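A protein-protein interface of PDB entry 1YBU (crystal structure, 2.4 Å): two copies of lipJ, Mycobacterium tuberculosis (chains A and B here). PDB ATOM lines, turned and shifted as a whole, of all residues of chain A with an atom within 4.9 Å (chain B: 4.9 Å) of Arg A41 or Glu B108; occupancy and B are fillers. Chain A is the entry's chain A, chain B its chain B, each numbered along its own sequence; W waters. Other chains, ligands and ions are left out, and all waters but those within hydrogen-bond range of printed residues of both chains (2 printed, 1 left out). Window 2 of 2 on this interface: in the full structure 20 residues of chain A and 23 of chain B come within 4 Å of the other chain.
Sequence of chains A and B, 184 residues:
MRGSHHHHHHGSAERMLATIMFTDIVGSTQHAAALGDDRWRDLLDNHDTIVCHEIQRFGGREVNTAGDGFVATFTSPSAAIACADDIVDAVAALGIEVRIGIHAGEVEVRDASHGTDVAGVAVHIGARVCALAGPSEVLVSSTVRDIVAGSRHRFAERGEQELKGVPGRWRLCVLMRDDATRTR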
ATOM      1  N   GLY A  36     -13.557 -20.022  18.810  1.00  0.00           N
ATOM      2  CA  GLY A  36     -12.305 -20.634  18.404  1.00  0.00           C
ATOM      3  C   GLY A  36     -12.436 -22.100  18.749  1.00  0.00           C
ATOM      4  O   GLY A  36     -13.225 -22.442  19.624  1.00  0.00           O
ATOM      5  N   ASP A  37     -11.691 -22.979  18.097  1.00  0.00           N
ATOM      6  CA  ASP A  37     -11.784 -24.409  18.361  1.00  0.00           C
ATOM      7  C   ASP A  37     -11.319 -24.829  19.752  1.00  0.00           C
ATOM      8  O   ASP A  37     -11.860 -25.771  20.332  1.00  0.00           O
ATOM      9  CB  ASP A  37     -10.985 -25.225  17.334  1.00  0.00           C
ATOM     10  CG  ASP A  37     -11.731 -25.427  16.022  1.00  0.00           C
ATOM     11  OD1 ASP A  37     -11.181 -26.131  15.147  1.00  0.00           O
ATOM     12  OD2 ASP A  37     -12.853 -24.888  15.860  1.00  0.00           O
ATOM     13  N   ASP A  38     -10.316 -24.148  20.294  1.00  0.00           N
ATOM     14  CA  ASP A  38      -9.803 -24.549  21.597  1.00  0.00           C
ATOM     15  C   ASP A  38     -10.834 -24.380  22.706  1.00  0.00           C
ATOM     16  O   ASP A  38     -11.065 -25.291  23.501  1.00  0.00           O
ATOM     17  CB  ASP A  38      -8.539 -23.765  21.937  1.00  0.00           C
ATOM     18  CG  ASP A  38      -7.811 -24.347  23.125  1.00  0.00           C
ATOM     19  OD1 ASP A  38      -7.574 -23.612  24.101  1.00  0.00           O
ATOM     20  OD2 ASP A  38      -7.476 -25.549  23.086  1.00  0.00           O
ATOM     21  N   ARG A  39     -11.454 -23.211  22.751  1.00  0.00           N
ATOM     22  CA  ARG A  39     -12.452 -22.955  23.764  1.00  0.00           C
ATOM     23  C   ARG A  39     -13.713 -23.740  23.464  1.00  0.00           C
ATOM     24  O   ARG A  39     -14.305 -24.316  24.378  1.00  0.00           O
ATOM     25  CB  ARG A  39     -12.729 -21.448  23.854  1.00  0.00           C
ATOM     26  CG  ARG A  39     -11.505 -20.703  24.389  1.00  0.00           C
ATOM     27  CD  ARG A  39     -11.779 -19.248  24.720  1.00  0.00           C
ATOM     28  NE  ARG A  39     -11.552 -18.382  23.575  1.00  0.00           N
ATOM     29  CZ  ARG A  39     -11.364 -17.071  23.664  1.00  0.00           C
ATOM     30  NH1 ARG A  39     -11.381 -16.476  24.848  1.00  0.00           N
ATOM     31  NH2 ARG A  39     -11.139 -16.357  22.572  1.00  0.00           N
ATOM     32  N   TRP A  40     -14.110 -23.790  22.194  1.00  0.00           N
ATOM     33  CA  TRP A  40     -15.293 -24.552  21.830  1.00  0.00           C
ATOM     34  C   TRP A  40     -15.119 -25.975  22.314  1.00  0.00           C
ATOM     35  O   TRP A  40     -16.012 -26.534  22.949  1.00  0.00           O
ATOM     36  CB  TRP A  40     -15.506 -24.569  20.336  1.00  0.00           C
ATOM     37  CG  TRP A  40     -16.568 -25.532  19.896  1.00  0.00           C
ATOM     38  CD1 TRP A  40     -16.385 -26.712  19.244  1.00  0.00           C
ATOM     39  CD2 TRP A  40     -17.973 -25.411  20.121  1.00  0.00           C
ATOM     40  NE1 TRP A  40     -17.590 -27.341  19.048  1.00  0.00           N
ATOM     41  CE2 TRP A  40     -18.583 -26.564  19.578  1.00  0.00           C
ATOM     42  CE3 TRP A  40     -18.778 -24.443  20.734  1.00  0.00           C
ATOM     43  CZ2 TRP A  40     -19.967 -26.776  19.630  1.00  0.00           C
ATOM     44  CZ3 TRP A  40     -20.152 -24.652  20.787  1.00  0.00           C
ATOM     45  CH2 TRP A  40     -20.732 -25.811  20.237  1.00  0.00           C
ATOM     46  N   ARG A  41     -13.967 -26.564  22.035  1.00  0.00           N
ATOM     47  CA  ARG A  41     -13.732 -27.925  22.475  1.00  0.00           C
ATOM     48  C   ARG A  41     -13.931 -28.070  23.974  1.00  0.00           C
ATOM     49  O   ARG A  41     -14.582 -29.007  24.436  1.00  0.00           O
ATOM     50  CB  ARG A  41     -12.316 -28.370  22.132  1.00  0.00           C
ATOM     51  CG  ARG A  41     -11.771 -29.463  23.050  1.00  0.00           C
ATOM     52  CD  ARG A  41     -10.249 -29.439  23.070  1.00  0.00           C
ATOM     53  NE  ARG A  41      -9.682 -30.091  24.250  1.00  0.00           N
ATOM     54  CZ  ARG A  41      -9.859 -31.372  24.563  1.00  0.00           C
ATOM     55  NH1 ARG A  41     -10.597 -32.154  23.784  1.00  0.00           N
ATOM     56  NH2 ARG A  41      -9.290 -31.876  25.652  1.00  0.00           N
ATOM     57  N   ASP A  42     -13.356 -27.159  24.744  1.00  0.00           N
ATOM     58  CA  ASP A  42     -13.493 -27.268  26.186  1.00  0.00           C
ATOM     59  C   ASP A  42     -14.932 -27.113  26.663  1.00  0.00           C
ATOM     60  O   ASP A  42     -15.371 -27.825  27.539  1.00  0.00           O
ATOM     61  CB  ASP A  42     -12.567 -26.273  26.881  1.00  0.00           C
ATOM     62  CG  ASP A  42     -11.187 -26.856  27.113  1.00  0.00           C
ATOM     63  OD1 ASP A  42     -11.046 -28.099  27.014  1.00  0.00           O
ATOM     64  OD2 ASP A  42     -10.251 -26.092  27.407  1.00  0.00           O
ATOM     65  N   LEU A  43     -15.651 -26.182  26.061  1.00  0.00           N
ATOM     66  CA  LEU A  43     -17.027 -25.935  26.377  1.00  0.00           C
ATOM     67  C   LEU A  43     -17.855 -27.198  26.088  1.00  0.00           C
ATOM     68  O   LEU A  43     -18.772 -27.533  26.847  1.00  0.00           O
ATOM     69  CB  LEU A  43     -17.518 -24.752  25.547  1.00  0.00           C
ATOM     70  CG  LEU A  43     -18.979 -24.350  25.691  1.00  0.00           C
ATOM     71  CD1 LEU A  43     -19.375 -24.399  27.153  1.00  0.00           C
ATOM     72  CD2 LEU A  43     -19.182 -22.958  25.112  1.00  0.00           C
ATOM     73  N   LEU A  44     -17.514 -27.900  25.008  1.00  0.00           N
ATOM     74  CA  LEU A  44     -18.209 -29.118  24.623  1.00  0.00           C
ATOM     75  C   LEU A  44     -18.022 -30.226  25.625  1.00  0.00           C
ATOM     76  O   LEU A  44     -18.979 -30.923  25.963  1.00  0.00           O
ATOM     77  CB  LEU A  44     -17.722 -29.637  23.266  1.00  0.00           C
ATOM     78  CG  LEU A  44     -18.543 -29.274  22.037  1.00  0.00           C
ATOM     79  CD1 LEU A  44     -17.965 -29.970  20.818  1.00  0.00           C
ATOM     80  CD2 LEU A  44     -19.974 -29.703  22.239  1.00  0.00           C
ATOM     81  N   ASP A  45     -16.795 -30.411  26.089  1.00  0.00           N
ATOM     82  CA  ASP A  45     -16.535 -31.477  27.042  1.00  0.00           C
ATOM     83  C   ASP A  45     -17.204 -31.210  28.369  1.00  0.00           C
ATOM     84  O   ASP A  45     -17.464 -32.134  29.135  1.00  0.00           O
ATOM     85  CB  ASP A  45     -15.031 -31.676  27.240  1.00  0.00           C
ATOM     86  CG  ASP A  45     -14.367 -32.274  26.016  1.00  0.00           C
ATOM     87  OD1 ASP A  45     -14.309 -31.606  24.970  1.00  0.00           O
ATOM     88  OD2 ASP A  45     -13.913 -33.408  26.080  1.00  0.00           O
ATOM     89  N   GLU B  14      -3.750 -33.232  19.748  1.00  0.00           N
ATOM     90  CA  GLU B  14      -3.999 -31.796  19.631  1.00  0.00           C
ATOM     91  C   GLU B  14      -4.797 -31.497  18.367  1.00  0.00           C
ATOM     92  O   GLU B  14      -5.672 -32.257  17.977  1.00  0.00           O
ATOM     93  CB  GLU B  14      -2.673 -31.034  19.589  1.00  0.00           C
ATOM     94  CG  GLU B  14      -2.818 -29.523  19.413  1.00  0.00           C
ATOM     95  CD  GLU B  14      -1.487 -28.806  19.332  1.00  0.00           C
ATOM     96  OE1 GLU B  14      -0.454 -29.415  19.692  1.00  0.00           O
ATOM     97  OE2 GLU B  14      -1.471 -27.622  18.932  1.00  0.00           O
ATOM     98  N   ARG B  15      -4.480 -30.366  17.751  1.00  0.00           N
ATOM     99  CA  ARG B  15      -5.114 -29.910  16.531  1.00  0.00           C
ATOM    100  C   ARG B  15      -4.529 -30.760  15.402  1.00  0.00           C
ATOM    101  O   ARG B  15      -3.317 -30.777  15.200  1.00  0.00           O
ATOM    102  CB  ARG B  15      -4.754 -28.446  16.281  1.00  0.00           C
ATOM    103  CG  ARG B  15      -5.674 -27.738  15.320  1.00  0.00           C
ATOM    104  CD  ARG B  15      -6.980 -27.360  15.991  1.00  0.00           C
ATOM    105  NE  ARG B  15      -7.905 -26.693  15.080  1.00  0.00           N
ATOM    106  CZ  ARG B  15      -7.591 -25.630  14.355  1.00  0.00           C
ATOM    107  NH1 ARG B  15      -6.372 -25.116  14.438  1.00  0.00           N
ATOM    108  NH2 ARG B  15      -8.492 -25.087  13.543  1.00  0.00           N
ATOM    109  N   GLU B 106      -8.379 -28.665  10.133  1.00  0.00           N
ATOM    110  CA  GLU B 106      -7.765 -29.099  11.377  1.00  0.00           C
ATOM    111  C   GLU B 106      -8.935 -29.273  12.345  1.00  0.00           C
ATOM    112  O   GLU B 106      -9.936 -28.564  12.246  1.00  0.00           O
ATOM    113  CB  GLU B 106      -6.785 -28.035  11.925  1.00  0.00           C
ATOM    114  CG  GLU B 106      -5.557 -27.746  11.042  1.00  0.00           C
ATOM    115  CD  GLU B 106      -4.508 -26.838  11.709  1.00  0.00           C
ATOM    116  OE1 GLU B 106      -4.830 -25.668  12.040  1.00  0.00           O
ATOM    117  OE2 GLU B 106      -3.358 -27.304  11.894  1.00  0.00           O
ATOM    118  N   VAL B 107      -8.821 -30.222  13.261  1.00  0.00           N
ATOM    119  CA  VAL B 107      -9.878 -30.439  14.228  1.00  0.00           C
ATOM    120  C   VAL B 107      -9.327 -30.810  15.593  1.00  0.00           C
ATOM    121  O   VAL B 107      -8.248 -31.406  15.710  1.00  0.00           O
ATOM    122  CB  VAL B 107     -10.880 -31.556  13.788  1.00  0.00           C
ATOM    123  CG1 VAL B 107     -11.621 -31.124  12.546  1.00  0.00           C
ATOM    124  CG2 VAL B 107     -10.151 -32.867  13.568  1.00  0.00           C
ATOM    125  N   GLU B 108     -10.093 -30.440  16.621  1.00  0.00           N
ATOM    126  CA  GLU B 108      -9.734 -30.737  18.000  1.00  0.00           C
ATOM    127  C   GLU B 108     -10.054 -32.188  18.239  1.00  0.00           C
ATOM    128  O   GLU B 108     -11.190 -32.598  18.062  1.00  0.00           O
ATOM    129  CB  GLU B 108     -10.547 -29.876  18.973  1.00  0.00           C
ATOM    130  CG  GLU B 108     -10.168 -28.401  18.989  1.00  0.00           C
ATOM    131  CD  GLU B 108      -8.723 -28.191  19.403  1.00  0.00           C
ATOM    132  OE1 GLU B 108      -8.317 -28.744  20.447  1.00  0.00           O
ATOM    133  OE2 GLU B 108      -8.009 -27.463  18.686  1.00  0.00           O
ATOM    134  N   VAL B 109      -9.063 -32.987  18.654  1.00  0.00           N
ATOM    135  CA  VAL B 109      -9.240 -34.429  18.893  1.00  0.00           C
ATOM    136  C   VAL B 109      -9.498 -34.702  20.317  1.00  0.00           C
ATOM    137  O   VAL B 109      -8.786 -34.171  21.171  1.00  0.00           O
ATOM    138  CB  VAL B 109      -8.045 -35.210  18.314  1.00  0.00           C
ATOM    139  CG1 VAL B 109      -8.227 -36.705  18.504  1.00  0.00           C
ATOM    140  CG2 VAL B 109      -7.873 -34.898  16.846  1.00  0.00           C
ATOM    141  N   ARG B 110     -10.513 -35.537  20.684  1.00  0.00           N
ATOM    142  CA  ARG B 110     -10.832 -35.700  22.141  1.00  0.00           C
ATOM    143  C   ARG B 110     -11.381 -36.993  22.766  1.00  0.00           C
ATOM    144  O   ARG B 110     -10.944 -38.112  22.484  1.00  0.00           O
ATOM    145  CB  ARG B 110     -11.816 -34.598  22.539  1.00  0.00           C
ATOM    146  CG  ARG B 110     -12.353 -33.785  21.360  1.00  0.00           C
ATOM    147  CD  ARG B 110     -13.660 -33.044  21.692  1.00  0.00           C
ATOM    148  NE  ARG B 110     -14.653 -33.922  22.315  1.00  0.00           N
ATOM    149  CZ  ARG B 110     -15.942 -33.627  22.448  1.00  0.00           C
ATOM    150  NH1 ARG B 110     -16.404 -32.470  21.983  1.00  0.00           N
ATOM    151  NH2 ARG B 110     -16.748 -34.484  23.056  1.00  0.00           N
ATOM    152  N   ASP B 117     -13.404 -39.244  19.215  1.00  0.00           N
ATOM    153  CA  ASP B 117     -14.271 -38.159  18.777  1.00  0.00           C
ATOM    154  C   ASP B 117     -13.455 -36.935  18.376  1.00  0.00           C
ATOM    155  O   ASP B 117     -12.325 -36.731  18.825  1.00  0.00           O
ATOM    156  CB  ASP B 117     -15.271 -37.791  19.877  1.00  0.00           C
ATOM    157  CG  ASP B 117     -16.462 -37.009  19.344  1.00  0.00           C
ATOM    158  OD1 ASP B 117     -16.254 -35.901  18.804  1.00  0.00           O
ATOM    159  OD2 ASP B 117     -17.609 -37.501  19.463  1.00  0.00           O
ATOM    160  N   VAL B 118     -14.052 -36.121  17.520  1.00  0.00           N
ATOM    161  CA  VAL B 118     -13.423 -34.924  16.992  1.00  0.00           C
ATOM    162  C   VAL B 118     -14.380 -33.751  17.137  1.00  0.00           C
ATOM    163  O   VAL B 118     -15.591 -33.952  17.259  1.00  0.00           O
ATOM    164  CB  VAL B 118     -13.059 -35.146  15.496  1.00  0.00           C
ATOM    165  CG1 VAL B 118     -13.177 -33.868  14.712  1.00  0.00           C
ATOM    166  CG2 VAL B 118     -11.655 -35.680  15.396  1.00  0.00           C
ATOM    167  N   ALA B 119     -13.832 -32.534  17.119  1.00  0.00           N
ATOM    168  CA  ALA B 119     -14.631 -31.324  17.260  1.00  0.00           C
ATOM    169  C   ALA B 119     -13.954 -30.076  16.693  1.00  0.00           C
ATOM    170  O   ALA B 119     -12.731 -29.971  16.670  1.00  0.00           O
ATOM    171  CB  ALA B 119     -14.950 -31.115  18.749  1.00  0.00           C
ATOM    172  N   GLY B 120     -14.768 -29.126  16.258  1.00  0.00           N
ATOM    173  CA  GLY B 120     -14.259 -27.881  15.736  1.00  0.00           C
ATOM    174  C   GLY B 120     -15.211 -27.425  14.673  1.00  0.00           C
ATOM    175  O   GLY B 120     -16.063 -28.197  14.252  1.00  0.00           O
HETATM  176  O   HOH W   1     -18.094 -29.581  16.681  1.00  0.00           O
HETATM  177  O   HOH W   2     -12.046 -27.384  13.223  1.00  0.00           O
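The side-chain carboxylate (OD1) of Asp A37 lies within salt-bridge range of the guanidinium group (NH2) of Arg B15 (3.3 Å).
The side-chain carboxylate (OD1) of Asp A45 is in salt-bridge range of the guanidinium group (NE) of Arg B110.
The side-chain carboxylate (OD1) of Asp A42 is in salt-bridge range of the guanidinium group (NE) of Arg A41, 3.7 Å away.
OD1 of Asp A45 is in salt-bridge range of NH1 of Arg A41, 3.9 Å away.
OE1 of Glu B106 lies within salt-bridge range of NH1 of Arg B15 (2.9 Å).
The guanidinium group (NE) of Arg B15 lies within salt-bridge range of the side-chain carboxylate (OE2) of Glu B108 (3.7 Å).
N of Glu B108 is in hydrogen-bond range of O of Ala B119.
N of Arg B110 lies within hydrogen-bond range of O of Asp B117, 2.9 Å away.
Among the printed residues, merely in contact across the chains: Asp A37 with Glu B106 (3.99 Å), Asp A37 with Glu B108 (3.4 Å), Asp A37 with Gly B120 (3.3 Å), Arg A41 with Glu B108 (3.3 Å), Arg A41 with Val B109 (3.8 Å), Arg A41 with Arg B110 (3.0 Å), Leu A44 with Arg B110 (3.2 Å) and Leu A44 with Ala B119 (3.8 Å).
Arg A41 touches just these residues of chain B: Glu B108 (3.3 Å), Val B109 (3.8 Å) and Arg B110 (3.0 Å).
Of chain A, only Asp A37 and Arg A41 come within 4 Å of Glu B108.
Of the printed residues of chain B, Asp A37 touches Arg B15, Glu B106, Glu B108 and Gly B120.
Of the printed residues of chain B, Leu A44 touches Arg B110 and Ala B119.
Of the printed residues of chain A, Glu B106 touches Asp A37.
Printed residues of chain A within 4 Å of Val B109: Arg A41.
Val B107 touches none of the printed residues of chain A.
Glu B14 touches none of the printed residues of chain A.
The nearest printed residue of chain B that does not touch Arg A41 is Ala B119 (5.1 Å).
The nearest residue of chain A that does not touch Glu B108 is Asp A38 (4.2 Å).
Printed residues of chain A that touch a printed residue of chain B: Asp A37, Arg A41, Leu A44 and Asp A45.
Hydrophobic or aromatic side chains of chain A that line the printed part of chain B: Leu A44.
Along chain B the printed residues that touch a printed residue of chain A span positions 15 to 120.
Among the printed residues, Asp or Glu carboxylates within 4 Å of a Lys or Arg side-chain nitrogen of the other chain: Asp A37 with Arg B15 and Asp A45 with Arg B110.
No position is printed for both chains.
Of the 10 pairs that touch across the chains among the printed residues, none has its exchanged pair printed and touching as well.
Water W2 bridges the side-chain carboxylate (OD1) of Asp A37 and the backbone carbonyl oxygen (O) of Glu B106.
Water W1 bridges the indole nitrogen of Trp A40 (3.3 Å) and the backbone NH of Gly B120 (3.4 Å).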
